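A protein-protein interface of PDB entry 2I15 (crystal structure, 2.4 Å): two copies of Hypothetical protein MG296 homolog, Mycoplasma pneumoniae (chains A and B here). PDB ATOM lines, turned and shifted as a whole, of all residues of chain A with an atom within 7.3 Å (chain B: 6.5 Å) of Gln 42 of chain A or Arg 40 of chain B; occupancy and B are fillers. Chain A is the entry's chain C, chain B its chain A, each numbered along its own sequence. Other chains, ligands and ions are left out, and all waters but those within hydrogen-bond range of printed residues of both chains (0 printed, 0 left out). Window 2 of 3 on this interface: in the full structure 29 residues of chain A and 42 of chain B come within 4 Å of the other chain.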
ATOM      1  N   ASN A  35     -28.986  -4.397  -8.661  1.00  0.00           N
ATOM      2  CA  ASN A  35     -27.626  -3.929  -8.476  1.00  0.00           C
ATOM      3  C   ASN A  35     -27.384  -3.407  -7.063  1.00  0.00           C
ATOM      4  O   ASN A  35     -26.328  -3.664  -6.483  1.00  0.00           O
ATOM      5  CB  ASN A  35     -27.304  -2.828  -9.479  1.00  0.00           C
ATOM      6  CG  ASN A  35     -26.878  -3.370 -10.823  1.00  0.00           C
ATOM      7  OD1 ASN A  35     -26.778  -4.579 -11.021  1.00  0.00           O
ATOM      8  ND2 ASN A  35     -26.616  -2.474 -11.754  1.00  0.00           N
ATOM      9  N   ARG A  36     -28.344  -2.659  -6.522  1.00  0.00           N
ATOM     10  CA  ARG A  36     -28.218  -2.112  -5.170  1.00  0.00           C
ATOM     11  C   ARG A  36     -28.195  -3.212  -4.120  1.00  0.00           C
ATOM     12  O   ARG A  36     -27.399  -3.150  -3.195  1.00  0.00           O
ATOM     13  CB  ARG A  36     -29.353  -1.127  -4.865  1.00  0.00           C
ATOM     14  CG  ARG A  36     -29.035   0.311  -5.257  1.00  0.00           C
ATOM     15  CD  ARG A  36     -30.216   1.236  -4.977  1.00  0.00           C
ATOM     16  NE  ARG A  36     -30.643   1.942  -6.185  1.00  0.00           N
ATOM     17  CZ  ARG A  36     -31.596   2.868  -6.216  1.00  0.00           C
ATOM     18  NH1 ARG A  36     -32.232   3.209  -5.102  1.00  0.00           N
ATOM     19  NH2 ARG A  36     -31.911   3.456  -7.363  1.00  0.00           N
ATOM     20  N   CYS A  37     -29.063  -4.211  -4.265  1.00  0.00           N
ATOM     21  CA  CYS A  37     -29.105  -5.332  -3.333  1.00  0.00           C
ATOM     22  C   CYS A  37     -27.765  -6.077  -3.394  1.00  0.00           C
ATOM     23  O   CYS A  37     -27.235  -6.522  -2.377  1.00  0.00           O
ATOM     24  CB  CYS A  37     -30.229  -6.296  -3.709  1.00  0.00           C
ATOM     25  SG  CYS A  37     -31.897  -5.636  -3.589  1.00  0.00           S
ATOM     26  N   LEU A  38     -27.223  -6.193  -4.603  1.00  0.00           N
ATOM     27  CA  LEU A  38     -25.966  -6.880  -4.824  1.00  0.00           C
ATOM     28  C   LEU A  38     -24.791  -6.220  -4.117  1.00  0.00           C
ATOM     29  O   LEU A  38     -24.031  -6.895  -3.418  1.00  0.00           O
ATOM     30  CB  LEU A  38     -25.665  -6.966  -6.320  1.00  0.00           C
ATOM     31  CG  LEU A  38     -25.319  -8.343  -6.888  1.00  0.00           C
ATOM     32  CD1 LEU A  38     -24.270  -8.168  -7.979  1.00  0.00           C
ATOM     33  CD2 LEU A  38     -24.795  -9.297  -5.814  1.00  0.00           C
ATOM     34  N   GLU A  39     -24.632  -4.912  -4.308  1.00  0.00           N
ATOM     35  CA  GLU A  39     -23.528  -4.204  -3.687  1.00  0.00           C
ATOM     36  C   GLU A  39     -23.647  -4.228  -2.183  1.00  0.00           C
ATOM     37  O   GLU A  39     -22.650  -4.315  -1.467  1.00  0.00           O
ATOM     38  CB  GLU A  39     -23.456  -2.746  -4.148  1.00  0.00           C
ATOM     39  CG  GLU A  39     -22.423  -1.963  -3.351  1.00  0.00           C
ATOM     40  CD  GLU A  39     -22.213  -0.557  -3.852  1.00  0.00           C
ATOM     41  OE1 GLU A  39     -23.205   0.208  -3.913  1.00  0.00           O
ATOM     42  OE2 GLU A  39     -21.051  -0.213  -4.177  1.00  0.00           O
ATOM     43  N   ARG A  40     -24.883  -4.147  -1.715  1.00  0.00           N
ATOM     44  CA  ARG A  40     -25.172  -4.146  -0.294  1.00  0.00           C
ATOM     45  C   ARG A  40     -24.842  -5.497   0.324  1.00  0.00           C
ATOM     46  O   ARG A  40     -24.468  -5.587   1.490  1.00  0.00           O
ATOM     47  CB  ARG A  40     -26.644  -3.823  -0.087  1.00  0.00           C
ATOM     48  CG  ARG A  40     -26.983  -3.511   1.322  1.00  0.00           C
ATOM     49  CD  ARG A  40     -28.456  -3.702   1.548  1.00  0.00           C
ATOM     50  NE  ARG A  40     -28.778  -3.657   2.961  1.00  0.00           N
ATOM     51  CZ  ARG A  40     -29.976  -3.918   3.459  1.00  0.00           C
ATOM     52  NH1 ARG A  40     -30.989  -4.249   2.654  1.00  0.00           N
ATOM     53  NH2 ARG A  40     -30.156  -3.844   4.770  1.00  0.00           N
ATOM     54  N   GLU A  41     -24.983  -6.550  -0.469  1.00  0.00           N
ATOM     55  CA  GLU A  41     -24.703  -7.905  -0.022  1.00  0.00           C
ATOM     56  C   GLU A  41     -23.205  -8.166  -0.003  1.00  0.00           C
ATOM     57  O   GLU A  41     -22.630  -8.555   1.013  1.00  0.00           O
ATOM     58  CB  GLU A  41     -25.342  -8.895  -0.974  1.00  0.00           C
ATOM     59  CG  GLU A  41     -24.874 -10.312  -0.748  1.00  0.00           C
ATOM     60  CD  GLU A  41     -25.935 -11.157  -0.113  1.00  0.00           C
ATOM     61  OE1 GLU A  41     -26.613 -10.665   0.823  1.00  0.00           O
ATOM     62  OE2 GLU A  41     -26.085 -12.314  -0.554  1.00  0.00           O
ATOM     63  N   GLN A  42     -22.582  -7.937  -1.150  1.00  0.00           N
ATOM     64  CA  GLN A  42     -21.168  -8.180  -1.328  1.00  0.00           C
ATOM     65  C   GLN A  42     -20.201  -7.280  -0.565  1.00  0.00           C
ATOM     66  O   GLN A  42     -19.003  -7.559  -0.542  1.00  0.00           O
ATOM     67  CB  GLN A  42     -20.890  -8.187  -2.834  1.00  0.00           C
ATOM     68  CG  GLN A  42     -21.817  -9.198  -3.489  1.00  0.00           C
ATOM     69  CD  GLN A  42     -21.588  -9.426  -4.954  1.00  0.00           C
ATOM     70  OE1 GLN A  42     -21.955 -10.475  -5.473  1.00  0.00           O
ATOM     71  NE2 GLN A  42     -21.007  -8.452  -5.642  1.00  0.00           N
ATOM     72  N   SER A  43     -20.711  -6.224   0.068  1.00  0.00           N
ATOM     73  CA  SER A  43     -19.868  -5.313   0.848  1.00  0.00           C
ATOM     74  C   SER A  43     -19.130  -6.033   1.984  1.00  0.00           C
ATOM     75  O   SER A  43     -17.973  -5.728   2.273  1.00  0.00           O
ATOM     76  CB  SER A  43     -20.716  -4.188   1.446  1.00  0.00           C
ATOM     77  OG  SER A  43     -21.303  -3.391   0.445  1.00  0.00           O
ATOM     78  N   THR A  44     -19.828  -6.967   2.630  1.00  0.00           N
ATOM     79  CA  THR A  44     -19.316  -7.783   3.741  1.00  0.00           C
ATOM     80  C   THR A  44     -18.403  -7.132   4.780  1.00  0.00           C
ATOM     81  O   THR A  44     -17.191  -7.351   4.769  1.00  0.00           O
ATOM     82  CB  THR A  44     -18.592  -9.068   3.208  1.00  0.00           C
ATOM     83  OG1 THR A  44     -17.524  -8.702   2.319  1.00  0.00           O
ATOM     84  CG2 THR A  44     -19.572  -9.971   2.475  1.00  0.00           C
ATOM     85  N   LEU A  45     -19.005  -6.361   5.683  1.00  0.00           N
ATOM     86  CA  LEU A  45     -18.292  -5.691   6.766  1.00  0.00           C
ATOM     87  C   LEU A  45     -19.296  -5.251   7.833  1.00  0.00           C
ATOM     88  O   LEU A  45     -19.122  -5.563   9.005  1.00  0.00           O
ATOM     89  CB  LEU A  45     -17.480  -4.496   6.240  1.00  0.00           C
ATOM     90  CG  LEU A  45     -15.971  -4.689   6.423  1.00  0.00           C
ATOM     91  CD1 LEU A  45     -15.215  -3.609   5.688  1.00  0.00           C
ATOM     92  CD2 LEU A  45     -15.629  -4.692   7.911  1.00  0.00           C
ATOM     93  N   ASP A  50     -26.932  -5.788   7.347  1.00  0.00           N
ATOM     94  CA  ASP A  50     -27.132  -6.133   5.957  1.00  0.00           C
ATOM     95  C   ASP A  50     -28.262  -7.115   5.799  1.00  0.00           C
ATOM     96  O   ASP A  50     -28.257  -8.149   6.466  1.00  0.00           O
ATOM     97  CB  ASP A  50     -25.873  -6.797   5.387  1.00  0.00           C
ATOM     98  CG  ASP A  50     -24.832  -5.812   4.991  1.00  0.00           C
ATOM     99  OD1 ASP A  50     -25.225  -4.734   4.510  1.00  0.00           O
ATOM    100  OD2 ASP A  50     -23.626  -6.107   5.129  1.00  0.00           O
ATOM    101  N   ASP A  52     -28.705  -9.665   4.802  1.00  0.00           N
ATOM    102  CA  ASP A  52     -27.705 -10.574   4.294  1.00  0.00           C
ATOM    103  C   ASP A  52     -28.418 -11.827   4.698  1.00  0.00           C
ATOM    104  O   ASP A  52     -29.648 -11.802   4.817  1.00  0.00           O
ATOM    105  CB  ASP A  52     -26.379 -10.379   5.051  1.00  0.00           C
ATOM    106  CG  ASP A  52     -25.178 -10.738   4.221  1.00  0.00           C
ATOM    107  OD1 ASP A  52     -25.080 -11.908   3.792  1.00  0.00           O
ATOM    108  OD2 ASP A  52     -24.327  -9.850   3.988  1.00  0.00           O
ATOM    109  N   PHE B  34     -10.571  -2.809 -13.214  1.00  0.00           N
ATOM    110  CA  PHE B  34     -11.253  -2.861 -14.491  1.00  0.00           C
ATOM    111  C   PHE B  34     -11.158  -4.273 -15.084  1.00  0.00           C
ATOM    112  O   PHE B  34     -12.175  -4.858 -15.472  1.00  0.00           O
ATOM    113  CB  PHE B  34     -10.641  -1.847 -15.454  1.00  0.00           C
ATOM    114  CG  PHE B  34     -11.245  -1.893 -16.823  1.00  0.00           C
ATOM    115  CD1 PHE B  34     -12.458  -1.259 -17.096  1.00  0.00           C
ATOM    116  CD2 PHE B  34     -10.644  -2.651 -17.819  1.00  0.00           C
ATOM    117  CE1 PHE B  34     -13.061  -1.396 -18.349  1.00  0.00           C
ATOM    118  CE2 PHE B  34     -11.239  -2.790 -19.056  1.00  0.00           C
ATOM    119  CZ  PHE B  34     -12.452  -2.165 -19.328  1.00  0.00           C
ATOM    120  N   ASN B  35      -9.942  -4.820 -15.148  1.00  0.00           N
ATOM    121  CA  ASN B  35      -9.754  -6.166 -15.692  1.00  0.00           C
ATOM    122  C   ASN B  35     -10.481  -7.196 -14.842  1.00  0.00           C
ATOM    123  O   ASN B  35     -10.929  -8.227 -15.344  1.00  0.00           O
ATOM    124  CB  ASN B  35      -8.260  -6.512 -15.782  1.00  0.00           C
ATOM    125  CG  ASN B  35      -7.552  -5.749 -16.894  1.00  0.00           C
ATOM    126  OD1 ASN B  35      -8.205  -5.181 -17.786  1.00  0.00           O
ATOM    127  ND2 ASN B  35      -6.212  -5.732 -16.856  1.00  0.00           N
ATOM    128  N   ARG B  36     -10.579  -6.927 -13.545  1.00  0.00           N
ATOM    129  CA  ARG B  36     -11.280  -7.837 -12.652  1.00  0.00           C
ATOM    130  C   ARG B  36     -12.778  -7.724 -12.889  1.00  0.00           C
ATOM    131  O   ARG B  36     -13.444  -8.734 -13.049  1.00  0.00           O
ATOM    132  CB  ARG B  36     -10.947  -7.546 -11.190  1.00  0.00           C
ATOM    133  CG  ARG B  36      -9.555  -7.992 -10.826  1.00  0.00           C
ATOM    134  CD  ARG B  36      -9.246  -7.717  -9.380  1.00  0.00           C
ATOM    135  NE  ARG B  36      -7.959  -7.054  -9.244  1.00  0.00           N
ATOM    136  CZ  ARG B  36      -7.270  -6.986  -8.114  1.00  0.00           C
ATOM    137  NH1 ARG B  36      -7.745  -7.547  -7.011  1.00  0.00           N
ATOM    138  NH2 ARG B  36      -6.105  -6.357  -8.086  1.00  0.00           N
ATOM    139  N   CYS B  37     -13.309  -6.503 -12.906  1.00  0.00           N
ATOM    140  CA  CYS B  37     -14.729  -6.303 -13.171  1.00  0.00           C
ATOM    141  C   CYS B  37     -15.097  -6.992 -14.482  1.00  0.00           C
ATOM    142  O   CYS B  37     -16.081  -7.731 -14.556  1.00  0.00           O
ATOM    143  CB  CYS B  37     -15.053  -4.815 -13.314  1.00  0.00           C
ATOM    144  SG  CYS B  37     -14.791  -3.766 -11.859  1.00  0.00           S
ATOM    145  N   LEU B  38     -14.302  -6.717 -15.517  1.00  0.00           N
ATOM    146  CA  LEU B  38     -14.499  -7.276 -16.858  1.00  0.00           C
ATOM    147  C   LEU B  38     -14.550  -8.798 -16.799  1.00  0.00           C
ATOM    148  O   LEU B  38     -15.562  -9.414 -17.138  1.00  0.00           O
ATOM    149  CB  LEU B  38     -13.342  -6.840 -17.778  1.00  0.00           C
ATOM    150  CG  LEU B  38     -13.647  -6.256 -19.157  1.00  0.00           C
ATOM    151  CD1 LEU B  38     -12.510  -6.629 -20.126  1.00  0.00           C
ATOM    152  CD2 LEU B  38     -14.997  -6.768 -19.684  1.00  0.00           C
ATOM    153  N   GLU B  39     -13.443  -9.392 -16.367  1.00  0.00           N
ATOM    154  CA  GLU B  39     -13.342 -10.833 -16.269  1.00  0.00           C
ATOM    155  C   GLU B  39     -14.565 -11.369 -15.535  1.00  0.00           C
ATOM    156  O   GLU B  39     -15.025 -12.480 -15.797  1.00  0.00           O
ATOM    157  CB  GLU B  39     -12.055 -11.199 -15.523  1.00  0.00           C
ATOM    158  CG  GLU B  39     -11.988 -12.614 -14.970  1.00  0.00           C
ATOM    159  CD  GLU B  39     -10.820 -12.804 -13.998  1.00  0.00           C
ATOM    160  OE1 GLU B  39     -10.664 -11.971 -13.069  1.00  0.00           O
ATOM    161  OE2 GLU B  39     -10.064 -13.787 -14.165  1.00  0.00           O
ATOM    162  N   ARG B  40     -15.096 -10.564 -14.625  1.00  0.00           N
ATOM    163  CA  ARG B  40     -16.254 -10.949 -13.833  1.00  0.00           C
ATOM    164  C   ARG B  40     -17.548 -10.874 -14.634  1.00  0.00           C
ATOM    165  O   ARG B  40     -18.429 -11.718 -14.495  1.00  0.00           O
ATOM    166  CB  ARG B  40     -16.369 -10.041 -12.611  1.00  0.00           C
ATOM    167  CG  ARG B  40     -17.394 -10.518 -11.627  1.00  0.00           C
ATOM    168  CD  ARG B  40     -17.592  -9.564 -10.468  1.00  0.00           C
ATOM    169  NE  ARG B  40     -18.629 -10.070  -9.577  1.00  0.00           N
ATOM    170  CZ  ARG B  40     -19.160  -9.382  -8.575  1.00  0.00           C
ATOM    171  NH1 ARG B  40     -18.748  -8.146  -8.322  1.00  0.00           N
ATOM    172  NH2 ARG B  40     -20.120  -9.927  -7.836  1.00  0.00           N
ATOM    173  N   GLU B  41     -17.644  -9.855 -15.474  1.00  0.00           N
ATOM    174  CA  GLU B  41     -18.814  -9.625 -16.300  1.00  0.00           C
ATOM    175  C   GLU B  41     -18.960 -10.658 -17.407  1.00  0.00           C
ATOM    176  O   GLU B  41     -20.081 -11.027 -17.793  1.00  0.00           O
ATOM    177  CB  GLU B  41     -18.713  -8.244 -16.938  1.00  0.00           C
ATOM    178  CG  GLU B  41     -19.935  -7.852 -17.746  1.00  0.00           C
ATOM    179  CD  GLU B  41     -21.133  -7.568 -16.863  1.00  0.00           C
ATOM    180  OE1 GLU B  41     -21.026  -7.730 -15.615  1.00  0.00           O
ATOM    181  OE2 GLU B  41     -22.182  -7.175 -17.424  1.00  0.00           O
ATOM    182  N   GLN B  42     -17.816 -11.119 -17.909  1.00  0.00           N
ATOM    183  CA  GLN B  42     -17.764 -12.064 -19.017  1.00  0.00           C
ATOM    184  C   GLN B  42     -17.598 -13.562 -18.705  1.00  0.00           C
ATOM    185  O   GLN B  42     -17.218 -14.330 -19.591  1.00  0.00           O
ATOM    186  CB  GLN B  42     -16.657 -11.613 -19.979  1.00  0.00           C
ATOM    187  CG  GLN B  42     -16.740 -10.137 -20.325  1.00  0.00           C
ATOM    188  CD  GLN B  42     -15.613  -9.660 -21.216  1.00  0.00           C
ATOM    189  OE1 GLN B  42     -15.782  -8.717 -21.980  1.00  0.00           O
ATOM    190  NE2 GLN B  42     -14.451 -10.294 -21.109  1.00  0.00           N
ATOM    191  N   SER B  43     -17.885 -13.987 -17.475  1.00  0.00           N
ATOM    192  CA  SER B  43     -17.760 -15.402 -17.123  1.00  0.00           C
ATOM    193  C   SER B  43     -18.920 -16.254 -17.647  1.00  0.00           C
ATOM    194  O   SER B  43     -18.746 -17.442 -17.939  1.00  0.00           O
ATOM    195  CB  SER B  43     -17.644 -15.575 -15.607  1.00  0.00           C
ATOM    196  OG  SER B  43     -17.764 -14.341 -14.921  1.00  0.00           O
ATOM    197  N   THR B  44     -20.091 -15.630 -17.762  1.00  0.00           N
ATOM    198  CA  THR B  44     -21.321 -16.259 -18.253  1.00  0.00           C
ATOM    199  C   THR B  44     -21.780 -17.572 -17.629  1.00  0.00           C
ATOM    200  O   THR B  44     -21.664 -18.636 -18.236  1.00  0.00           O
ATOM    201  CB  THR B  44     -21.271 -16.458 -19.780  1.00  0.00           C
ATOM    202  OG1 THR B  44     -20.038 -17.089 -20.144  1.00  0.00           O
ATOM    203  CG2 THR B  44     -21.398 -15.126 -20.493  1.00  0.00           C
ATOM    204  N   GLU B  49     -25.409 -13.227  -9.317  1.00  0.00           N
ATOM    205  CA  GLU B  49     -24.625 -12.682  -8.204  1.00  0.00           C
ATOM    206  C   GLU B  49     -23.623 -11.741  -8.830  1.00  0.00           C
ATOM    207  O   GLU B  49     -22.825 -11.077  -8.160  1.00  0.00           O
ATOM    208  CB  GLU B  49     -23.854 -13.788  -7.503  1.00  0.00           C
ATOM    209  CG  GLU B  49     -24.761 -14.912  -7.074  1.00  0.00           C
ATOM    210  CD  GLU B  49     -25.021 -14.864  -5.604  1.00  0.00           C
ATOM    211  OE1 GLU B  49     -24.225 -15.473  -4.857  1.00  0.00           O
ATOM    212  OE2 GLU B  49     -25.989 -14.187  -5.200  1.00  0.00           O
ATOM    213  N   ASP B  50     -23.674 -11.737 -10.149  1.00  0.00           N
ATOM    214  CA  ASP B  50     -22.797 -10.967 -10.971  1.00  0.00           C
ATOM    215  C   ASP B  50     -23.056  -9.505 -10.857  1.00  0.00           C
ATOM    216  O   ASP B  50     -24.169  -9.063 -11.187  1.00  0.00           O
ATOM    217  CB  ASP B  50     -22.987 -11.391 -12.435  1.00  0.00           C
ATOM    218  CG  ASP B  50     -21.695 -11.507 -13.179  1.00  0.00           C
ATOM    219  OD1 ASP B  50     -20.935 -10.516 -13.229  1.00  0.00           O
ATOM    220  OD2 ASP B  50     -21.449 -12.601 -13.724  1.00  0.00           O
ATOM    221  N   ASP B  51     -22.070  -8.745 -10.371  1.00  0.00           N
ATOM    222  CA  ASP B  51     -22.291  -7.319 -10.401  1.00  0.00           C
ATOM    223  C   ASP B  51     -22.319  -7.443 -11.911  1.00  0.00           C
ATOM    224  O   ASP B  51     -21.322  -7.789 -12.562  1.00  0.00           O
ATOM    225  CB  ASP B  51     -21.086  -6.499  -9.939  1.00  0.00           C
ATOM    226  CG  ASP B  51     -21.362  -5.024  -9.977  1.00  0.00           C
ATOM    227  OD1 ASP B  51     -20.406  -4.229  -9.838  1.00  0.00           O
ATOM    228  OD2 ASP B  51     -22.538  -4.651 -10.151  1.00  0.00           O
ATOM    229  N   ASP B  52     -23.504  -7.243 -12.454  1.00  0.00           N
ATOM    230  CA  ASP B  52     -23.738  -7.411 -13.873  1.00  0.00           C
ATOM    231  C   ASP B  52     -24.927  -6.511 -13.894  1.00  0.00           C
ATOM    232  O   ASP B  52     -25.217  -5.899 -12.869  1.00  0.00           O
ATOM    233  CB  ASP B  52     -24.129  -8.886 -14.083  1.00  0.00           C
ATOM    234  CG  ASP B  52     -24.006  -9.367 -15.519  1.00  0.00           C
ATOM    235  OD1 ASP B  52     -24.699  -8.835 -16.401  1.00  0.00           O
ATOM    236  OD2 ASP B  52     -23.222 -10.313 -15.761  1.00  0.00           O
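NH2 of Arg 40 of chain B lies close to NE2 of Gln 42 of chain A. The backbone carbonyl oxygen (O) of Glu 49 of chain B sits close to the side-chain amide oxygen (OE1) of Gln 42 of chain A, at 2.9 Å. The backbone carbonyl oxygen (O) of Asp 52 of chain B sits close to the side-chain amide oxygen (OD1) of Asn 35 of chain A (2.8 Å).
O of Arg 40 of chain B is in hydrogen-bond range of OG of Ser 43 of chain B (2.7 Å). NH2 of Arg 40 of chain B is in hydrogen-bond range of O of Glu 49 of chain B (3.0 Å). O of Gln 42 of chain A lies within hydrogen-bond range of OG1 of Thr 44 of chain A (3.4 Å).
Among the printed residues, merely in contact across the chains: Leu 38 of chain A with Asp 51 of chain B (3.2 Å), Leu 38 of chain A with Glu 49 of chain B (3.3 Å) and Leu 38 of chain A with Asp 50 of chain B (3.3 Å).
Cys 37 of chain A touches none of the printed residues of chain B. Gln 42 of chain A touches just these residues of chain B: Arg 40 (2.8 Å) and Glu 49 (2.9 Å). Arg 40 of chain B touches one residue of chain A. Gln 42 of chain B touches none of the printed residues of chain A. Of the printed residues of chain A, Glu 49 of chain B touches Leu 38 and Gln 42. Of the printed residues of chain A, Asp 50 of chain B touches Leu 38 (3.3 Å). Of the printed residues of chain A, Asp 51 of chain B touches Leu 38. The nearest residue of chain B that does not touch Gln 42 of chain A is Asp 51 of chain B (4.7 Å).
Printed residues of chain B that touch a printed residue of chain A: Arg 40, Glu 49, Asp 50, Asp 51 and Asp 52. Hydrophobic or aromatic side chains of chain A that line the printed part of chain B: Leu 38. Among the printed residues, 6 pairs touch across the chains. Among the printed residues, no Asp or Glu carboxylate lies within 4 Å of a Lys or Arg side-chain nitrogen of the other chain.
Asn 35 of chain A touches Asp 52 of chain B, but with the chains exchanged Asp 52 of chain A does not touch Asn 35 of chain B (23.5 Å). Leu 38 of chain A touches Asp 50 of chain B, but with the chains exchanged Asp 50 of chain A does not touch Leu 38 of chain B (22.7 Å). Gln 42 of chain A touches Arg 40 of chain B, but with the chains exchanged Arg 40 of chain A does not touch Gln 42 of chain B (19.0 Å). Positions printed for both chains: 35, 36, 37, 38, 39, 40, 41, 42, 43, 44, 50 and 52. Of the 6 pairs that touch across the chains among the printed residues, none has its exchanged pair printed and touching as well.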
